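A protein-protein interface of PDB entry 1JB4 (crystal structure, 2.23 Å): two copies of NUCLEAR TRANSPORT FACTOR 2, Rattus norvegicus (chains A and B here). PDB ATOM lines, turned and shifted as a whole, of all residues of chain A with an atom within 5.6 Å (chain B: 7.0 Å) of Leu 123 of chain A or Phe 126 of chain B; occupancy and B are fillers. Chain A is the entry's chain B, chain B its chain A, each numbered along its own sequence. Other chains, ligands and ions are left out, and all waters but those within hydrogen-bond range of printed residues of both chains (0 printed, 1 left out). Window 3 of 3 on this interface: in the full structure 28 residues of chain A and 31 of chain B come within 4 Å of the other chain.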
ATOM      1  N   HIS A 100      19.097 -28.434  16.757  1.00  0.00           N
ATOM      2  CA  HIS A 100      19.356 -27.870  18.066  1.00  0.00           C
ATOM      3  C   HIS A 100      18.109 -27.100  18.443  1.00  0.00           C
ATOM      4  O   HIS A 100      17.597 -26.305  17.656  1.00  0.00           O
ATOM      5  CB  HIS A 100      20.556 -26.933  17.987  1.00  0.00           C
ATOM      6  CG  HIS A 100      21.810 -27.613  17.549  1.00  0.00           C
ATOM      7  ND1 HIS A 100      22.686 -28.204  18.437  1.00  0.00           N
ATOM      8  CD2 HIS A 100      22.315 -27.838  16.314  1.00  0.00           C
ATOM      9  CE1 HIS A 100      23.678 -28.761  17.764  1.00  0.00           C
ATOM     10  NE2 HIS A 100      23.476 -28.554  16.474  1.00  0.00           N
ATOM     11  N   ARG A 120      17.098 -24.633  15.195  1.00  0.00           N
ATOM     12  CA  ARG A 120      18.044 -24.480  14.082  1.00  0.00           C
ATOM     13  C   ARG A 120      18.530 -25.832  13.583  1.00  0.00           C
ATOM     14  O   ARG A 120      18.658 -26.789  14.341  1.00  0.00           O
ATOM     15  CB  ARG A 120      19.271 -23.650  14.470  1.00  0.00           C
ATOM     16  CG  ARG A 120      19.096 -22.153  14.314  1.00  0.00           C
ATOM     17  CD  ARG A 120      20.439 -21.434  14.408  1.00  0.00           C
ATOM     18  NE  ARG A 120      20.254 -19.996  14.287  1.00  0.00           N
ATOM     19  CZ  ARG A 120      19.921 -19.369  13.164  1.00  0.00           C
ATOM     20  NH1 ARG A 120      19.743 -20.046  12.042  1.00  0.00           N
ATOM     21  NH2 ARG A 120      19.716 -18.063  13.181  1.00  0.00           N
ATOM     22  N   LEU A 121      18.797 -25.898  12.290  1.00  0.00           N
ATOM     23  CA  LEU A 121      19.297 -27.114  11.675  1.00  0.00           C
ATOM     24  C   LEU A 121      20.786 -26.935  11.446  1.00  0.00           C
ATOM     25  O   LEU A 121      21.253 -25.824  11.192  1.00  0.00           O
ATOM     26  CB  LEU A 121      18.622 -27.354  10.329  1.00  0.00           C
ATOM     27  CG  LEU A 121      17.141 -27.723  10.285  1.00  0.00           C
ATOM     28  CD1 LEU A 121      16.645 -27.538   8.853  1.00  0.00           C
ATOM     29  CD2 LEU A 121      16.931 -29.168  10.777  1.00  0.00           C
ATOM     30  N   ALA A 122      21.528 -28.032  11.544  1.00  0.00           N
ATOM     31  CA  ALA A 122      22.962 -28.001  11.319  1.00  0.00           C
ATOM     32  C   ALA A 122      23.147 -28.269   9.837  1.00  0.00           C
ATOM     33  O   ALA A 122      22.525 -29.183   9.311  1.00  0.00           O
ATOM     34  CB  ALA A 122      23.633 -29.086  12.132  1.00  0.00           C
ATOM     35  N   LEU A 123      23.956 -27.464   9.152  1.00  0.00           N
ATOM     36  CA  LEU A 123      24.193 -27.696   7.728  1.00  0.00           C
ATOM     37  C   LEU A 123      24.890 -29.051   7.676  1.00  0.00           C
ATOM     38  O   LEU A 123      26.093 -29.134   7.919  1.00  0.00           O
ATOM     39  CB  LEU A 123      25.101 -26.607   7.139  1.00  0.00           C
ATOM     40  CG  LEU A 123      24.532 -25.187   7.065  1.00  0.00           C
ATOM     41  CD1 LEU A 123      25.112 -24.468   5.843  1.00  0.00           C
ATOM     42  CD2 LEU A 123      23.010 -25.250   6.952  1.00  0.00           C
ATOM     43  N   HIS A 124      24.138 -30.107   7.358  1.00  0.00           N
ATOM     44  CA  HIS A 124      24.688 -31.462   7.352  1.00  0.00           C
ATOM     45  C   HIS A 124      25.471 -31.949   6.129  1.00  0.00           C
ATOM     46  O   HIS A 124      25.268 -31.498   5.001  1.00  0.00           O
ATOM     47  CB  HIS A 124      23.583 -32.480   7.662  1.00  0.00           C
ATOM     48  CG  HIS A 124      24.085 -33.735   8.313  1.00  0.00           C
ATOM     49  ND1 HIS A 124      25.338 -34.253   8.065  1.00  0.00           N
ATOM     50  CD2 HIS A 124      23.501 -34.581   9.196  1.00  0.00           C
ATOM     51  CE1 HIS A 124      25.507 -35.361   8.769  1.00  0.00           C
ATOM     52  NE2 HIS A 124      24.407 -35.584   9.463  1.00  0.00           N
ATOM     53  N   ASN A 125      26.363 -32.898   6.405  1.00  0.00           N
ATOM     54  CA  ASN A 125      27.247 -33.531   5.434  1.00  0.00           C
ATOM     55  C   ASN A 125      27.109 -35.036   5.674  1.00  0.00           C
ATOM     56  O   ASN A 125      26.397 -35.448   6.562  1.00  0.00           O
ATOM     57  CB  ASN A 125      28.678 -33.086   5.707  1.00  0.00           C
ATOM     58  CG  ASN A 125      28.737 -31.755   6.438  1.00  0.00           C
ATOM     59  OD1 ASN A 125      28.246 -30.739   5.939  1.00  0.00           O
ATOM     60  ND2 ASN A 125      29.329 -31.755   7.629  1.00  0.00           N
ATOM     61  N   THR B  69      28.512 -17.776  14.478  1.00  0.00           N
ATOM     62  CA  THR B  69      27.915 -17.930  13.159  1.00  0.00           C
ATOM     63  C   THR B  69      26.544 -17.271  13.198  1.00  0.00           C
ATOM     64  O   THR B  69      26.189 -16.503  12.305  1.00  0.00           O
ATOM     65  CB  THR B  69      27.749 -19.418  12.761  1.00  0.00           C
ATOM     66  OG1 THR B  69      29.040 -20.022  12.590  1.00  0.00           O
ATOM     67  CG2 THR B  69      26.986 -19.532  11.451  1.00  0.00           C
ATOM     68  N   ALA B  70      25.787 -17.574  14.249  1.00  0.00           N
ATOM     69  CA  ALA B  70      24.454 -17.012  14.419  1.00  0.00           C
ATOM     70  C   ALA B  70      24.054 -16.905  15.884  1.00  0.00           C
ATOM     71  O   ALA B  70      24.504 -17.697  16.730  1.00  0.00           O
ATOM     72  CB  ALA B  70      23.422 -17.864  13.667  1.00  0.00           C
ATOM     73  N   MET B  84      20.037 -18.014  21.883  1.00  0.00           N
ATOM     74  CA  MET B  84      20.619 -19.190  21.260  1.00  0.00           C
ATOM     75  C   MET B  84      21.852 -18.721  20.483  1.00  0.00           C
ATOM     76  O   MET B  84      21.812 -17.719  19.771  1.00  0.00           O
ATOM     77  CB  MET B  84      19.623 -19.868  20.316  1.00  0.00           C
ATOM     78  CG  MET B  84      20.163 -21.184  19.761  1.00  0.00           C
ATOM     79  SD  MET B  84      18.922 -22.275  19.034  1.00  0.00           S
ATOM     80  CE  MET B  84      19.956 -23.337  18.058  1.00  0.00           C
ATOM     81  N   VAL B  85      22.957 -19.432  20.648  1.00  0.00           N
ATOM     82  CA  VAL B  85      24.187 -19.079  19.959  1.00  0.00           C
ATOM     83  C   VAL B  85      24.834 -20.309  19.326  1.00  0.00           C
ATOM     84  O   VAL B  85      25.000 -21.332  19.985  1.00  0.00           O
ATOM     85  CB  VAL B  85      25.184 -18.439  20.939  1.00  0.00           C
ATOM     86  CG1 VAL B  85      26.560 -18.393  20.318  1.00  0.00           C
ATOM     87  CG2 VAL B  85      24.717 -17.042  21.315  1.00  0.00           C
ATOM     88  N   VAL B  86      25.181 -20.199  18.042  1.00  0.00           N
ATOM     89  CA  VAL B  86      25.825 -21.279  17.307  1.00  0.00           C
ATOM     90  C   VAL B  86      27.027 -20.725  16.547  1.00  0.00           C
ATOM     91  O   VAL B  86      27.027 -19.571  16.131  1.00  0.00           O
ATOM     92  CB  VAL B  86      24.833 -21.978  16.326  1.00  0.00           C
ATOM     93  CG1 VAL B  86      23.762 -22.716  17.124  1.00  0.00           C
ATOM     94  CG2 VAL B  86      24.190 -20.954  15.387  1.00  0.00           C
ATOM     95  N   GLY B  87      28.058 -21.546  16.388  1.00  0.00           N
ATOM     96  CA  GLY B  87      29.260 -21.112  15.695  1.00  0.00           C
ATOM     97  C   GLY B  87      30.400 -22.079  15.959  1.00  0.00           C
ATOM     98  O   GLY B  87      30.165 -23.248  16.298  1.00  0.00           O
ATOM     99  N   GLN B  88      31.638 -21.614  15.822  1.00  0.00           N
ATOM    100  CA  GLN B  88      32.777 -22.507  16.048  1.00  0.00           C
ATOM    101  C   GLN B  88      33.760 -21.989  17.097  1.00  0.00           C
ATOM    102  O   GLN B  88      33.871 -20.789  17.322  1.00  0.00           O
ATOM    103  CB  GLN B  88      33.534 -22.743  14.733  1.00  0.00           C
ATOM    104  CG  GLN B  88      32.756 -22.403  13.467  1.00  0.00           C
ATOM    105  CD  GLN B  88      33.643 -22.412  12.228  1.00  0.00           C
ATOM    106  OE1 GLN B  88      34.782 -21.924  12.259  1.00  0.00           O
ATOM    107  NE2 GLN B  88      33.123 -22.955  11.127  1.00  0.00           N
ATOM    108  N   GLY B  98      32.288 -27.139  16.508  1.00  0.00           N
ATOM    109  CA  GLY B  98      31.052 -26.400  16.438  1.00  0.00           C
ATOM    110  C   GLY B  98      30.495 -26.420  17.836  1.00  0.00           C
ATOM    111  O   GLY B  98      30.848 -27.300  18.625  1.00  0.00           O
ATOM    112  N   PHE B  99      29.649 -25.452  18.162  1.00  0.00           N
ATOM    113  CA  PHE B  99      29.047 -25.424  19.484  1.00  0.00           C
ATOM    114  C   PHE B  99      27.688 -24.731  19.474  1.00  0.00           C
ATOM    115  O   PHE B  99      27.376 -23.910  18.602  1.00  0.00           O
ATOM    116  CB  PHE B  99      29.979 -24.726  20.491  1.00  0.00           C
ATOM    117  CG  PHE B  99      29.941 -23.234  20.409  1.00  0.00           C
ATOM    118  CD1 PHE B  99      28.982 -22.503  21.116  1.00  0.00           C
ATOM    119  CD2 PHE B  99      30.820 -22.559  19.584  1.00  0.00           C
ATOM    120  CE1 PHE B  99      28.895 -21.118  21.001  1.00  0.00           C
ATOM    121  CE2 PHE B  99      30.745 -21.171  19.457  1.00  0.00           C
ATOM    122  CZ  PHE B  99      29.770 -20.447  20.174  1.00  0.00           C
ATOM    123  N   HIS B 100      26.889 -25.102  20.462  1.00  0.00           N
ATOM    124  CA  HIS B 100      25.573 -24.551  20.682  1.00  0.00           C
ATOM    125  C   HIS B 100      25.583 -24.073  22.139  1.00  0.00           C
ATOM    126  O   HIS B 100      25.963 -24.829  23.046  1.00  0.00           O
ATOM    127  CB  HIS B 100      24.509 -25.637  20.500  1.00  0.00           C
ATOM    128  CG  HIS B 100      23.126 -25.207  20.888  1.00  0.00           C
ATOM    129  ND1 HIS B 100      22.040 -26.051  20.813  1.00  0.00           N
ATOM    130  CD2 HIS B 100      22.654 -24.032  21.370  1.00  0.00           C
ATOM    131  CE1 HIS B 100      20.960 -25.415  21.235  1.00  0.00           C
ATOM    132  NE2 HIS B 100      21.307 -24.189  21.580  1.00  0.00           N
ATOM    133  N   ALA B 122      29.712 -29.608  19.084  1.00  0.00           N
ATOM    134  CA  ALA B 122      28.999 -30.240  18.003  1.00  0.00           C
ATOM    135  C   ALA B 122      29.917 -30.460  16.837  1.00  0.00           C
ATOM    136  O   ALA B 122      30.784 -29.635  16.557  1.00  0.00           O
ATOM    137  CB  ALA B 122      27.813 -29.377  17.581  1.00  0.00           C
ATOM    138  N   LEU B 123      29.718 -31.592  16.172  1.00  0.00           N
ATOM    139  CA  LEU B 123      30.485 -31.961  14.997  1.00  0.00           C
ATOM    140  C   LEU B 123      29.747 -31.411  13.774  1.00  0.00           C
ATOM    141  O   LEU B 123      30.011 -31.809  12.635  1.00  0.00           O
ATOM    142  CB  LEU B 123      30.580 -33.479  14.912  1.00  0.00           C
ATOM    143  CG  LEU B 123      31.309 -34.141  16.077  1.00  0.00           C
ATOM    144  CD1 LEU B 123      31.118 -35.637  16.017  1.00  0.00           C
ATOM    145  CD2 LEU B 123      32.786 -33.773  16.014  1.00  0.00           C
ATOM    146  N   HIS B 124      28.815 -30.495  14.025  1.00  0.00           N
ATOM    147  CA  HIS B 124      28.024 -29.881  12.964  1.00  0.00           C
ATOM    148  C   HIS B 124      28.672 -28.582  12.542  1.00  0.00           C
ATOM    149  O   HIS B 124      29.747 -28.218  13.006  1.00  0.00           O
ATOM    150  CB  HIS B 124      26.622 -29.521  13.453  1.00  0.00           C
ATOM    151  CG  HIS B 124      25.883 -30.643  14.105  1.00  0.00           C
ATOM    152  ND1 HIS B 124      24.903 -30.428  15.049  1.00  0.00           N
ATOM    153  CD2 HIS B 124      25.941 -31.983  13.923  1.00  0.00           C
ATOM    154  CE1 HIS B 124      24.389 -31.583  15.424  1.00  0.00           C
ATOM    155  NE2 HIS B 124      25.001 -32.544  14.756  1.00  0.00           N
ATOM    156  N   ASN B 125      27.969 -27.876  11.671  1.00  0.00           N
ATOM    157  CA  ASN B 125      28.386 -26.583  11.174  1.00  0.00           C
ATOM    158  C   ASN B 125      27.058 -25.882  10.918  1.00  0.00           C
ATOM    159  O   ASN B 125      26.032 -26.553  10.766  1.00  0.00           O
ATOM    160  CB  ASN B 125      29.155 -26.736   9.870  1.00  0.00           C
ATOM    161  CG  ASN B 125      30.041 -25.552   9.584  1.00  0.00           C
ATOM    162  OD1 ASN B 125      30.434 -25.324   8.442  1.00  0.00           O
ATOM    163  ND2 ASN B 125      30.375 -24.796  10.626  1.00  0.00           N
ATOM    164  N   PHE B 126      27.061 -24.554  10.862  1.00  0.00           N
ATOM    165  CA  PHE B 126      25.817 -23.830  10.634  1.00  0.00           C
ATOM    166  C   PHE B 126      25.894 -22.791   9.521  1.00  0.00           C
ATOM    167  O   PHE B 126      26.993 -22.612   8.958  1.00  0.00           O
ATOM    168  CB  PHE B 126      25.365 -23.164  11.931  1.00  0.00           C
ATOM    169  CG  PHE B 126      25.365 -24.089  13.112  1.00  0.00           C
ATOM    170  CD1 PHE B 126      26.554 -24.393  13.773  1.00  0.00           C
ATOM    171  CD2 PHE B 126      24.181 -24.664  13.561  1.00  0.00           C
ATOM    172  CE1 PHE B 126      26.565 -25.253  14.865  1.00  0.00           C
ATOM    173  CE2 PHE B 126      24.182 -25.526  14.653  1.00  0.00           C
ATOM    174  CZ  PHE B 126      25.372 -25.819  15.305  1.00  0.00           C
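N of Thr 69 of chain B sits at hydrogen-bond distance from O of Val 86 of chain B, at 2.9 Å. O of Ala 70 of chain B is in hydrogen-bond range of N of Val 86 of chain B, at 2.9 Å. The side-chain amide nitrogen (ND2) of Asn 125 of chain B sits close to the side-chain amide nitrogen (NE2) of Gln 88 of chain B (3.3 Å). The backbone carbonyl oxygen (O) of Arg 120 of chain A sits at hydrogen-bond distance from the backbone NH (N) of His 100 of chain A, 3.0 Å away. The backbone carbonyl oxygen (O) of Leu 123 of chain A sits close to the side-chain amide oxygen (OD1) of Asn 125 of chain A (3.3 Å).
Printed residues of chain B that touch a printed residue of chain A: Ala 70, Met 84, Val 86, His 100, His 124, Asn 125 and Phe 126. Along chain B the printed residues that touch a printed residue of chain A span positions 70 to 126.
His 100 of chain A touches its own counterpart, His 100 of chain B. Ala 122 of chain A touches His 124 of chain B, but with the chains exchanged His 124 of chain A does not touch Ala 122 of chain B (10.4 Å). Ala 122 of chain A touches Asn 125 of chain B, but with the chains exchanged Asn 125 of chain A does not touch Ala 122 of chain B (9.3 Å). Leu 123 of chain A touches Asn 125 of chain B, but with the chains exchanged Asn 125 of chain A does not touch Leu 123 of chain B (5.1 Å). Positions printed for both chains: 100, 122, 123, 124 and 125. Of the 12 pairs that touch across the chains among the printed residues, 1 has its exchanged pair printed and touching as well.
Among the printed residues, pairs that only touch across the chains: Ala 122 of chain A with His 124 of chain B (3.3 Å), His 100 of chain A with Phe 126 of chain B (3.4 Å), Ala 122 of chain A with Asn 125 of chain B (3.4 Å), His 100 of chain A with Met 84 of chain B (3.6 Å), Arg 120 of chain A with Met 84 of chain B (3.7 Å), Leu 123 of chain A with Phe 126 of chain B (3.7 Å), Arg 120 of chain A with Ala 70 of chain B (3.7 Å), Arg 120 of chain A with Val 86 of chain B (3.9 Å) and Leu 121 of chain A with Phe 126 of chain B (3.9 Å).
Of the printed residues of chain B, Leu 123 of chain A touches Asn 125 and Phe 126. Of chain A, only His 100 (3.4 Å), Leu 121 (3.9 Å) and Leu 123 (3.7 Å) come within 4 Å of Phe 126 of chain B. Printed residues of chain B within 4 Å of His 100 of chain A: Met 84, His 100, His 124 and Phe 126. Printed residues of chain A within 4 Å of His 100 of chain B: His 100 (3.3 Å). Printed residues of chain A within 4 Å of His 124 of chain B: His 100 (2.8 Å) and Ala 122 (3.3 Å). Of the printed residues of chain B, Leu 121 of chain A touches Phe 126 (3.9 Å). Thr 69 of chain B touches none of the printed residues of chain A. Ala 122 of chain B touches none of the printed residues of chain A.
ND1 of His 100 of chain B sits at hydrogen-bond distance from ND1 of His 100 of chain A, at 3.3 Å. A ring nitrogen (ND1) of His 124 of chain B lies within hydrogen-bond range of a ring nitrogen (NE2) of His 100 of chain A, at 2.8 Å. The backbone carbonyl oxygen of Asn 125 of chain B is in hydrogen-bond range of the backbone NH of Leu 123 of chain A (2.8 Å).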
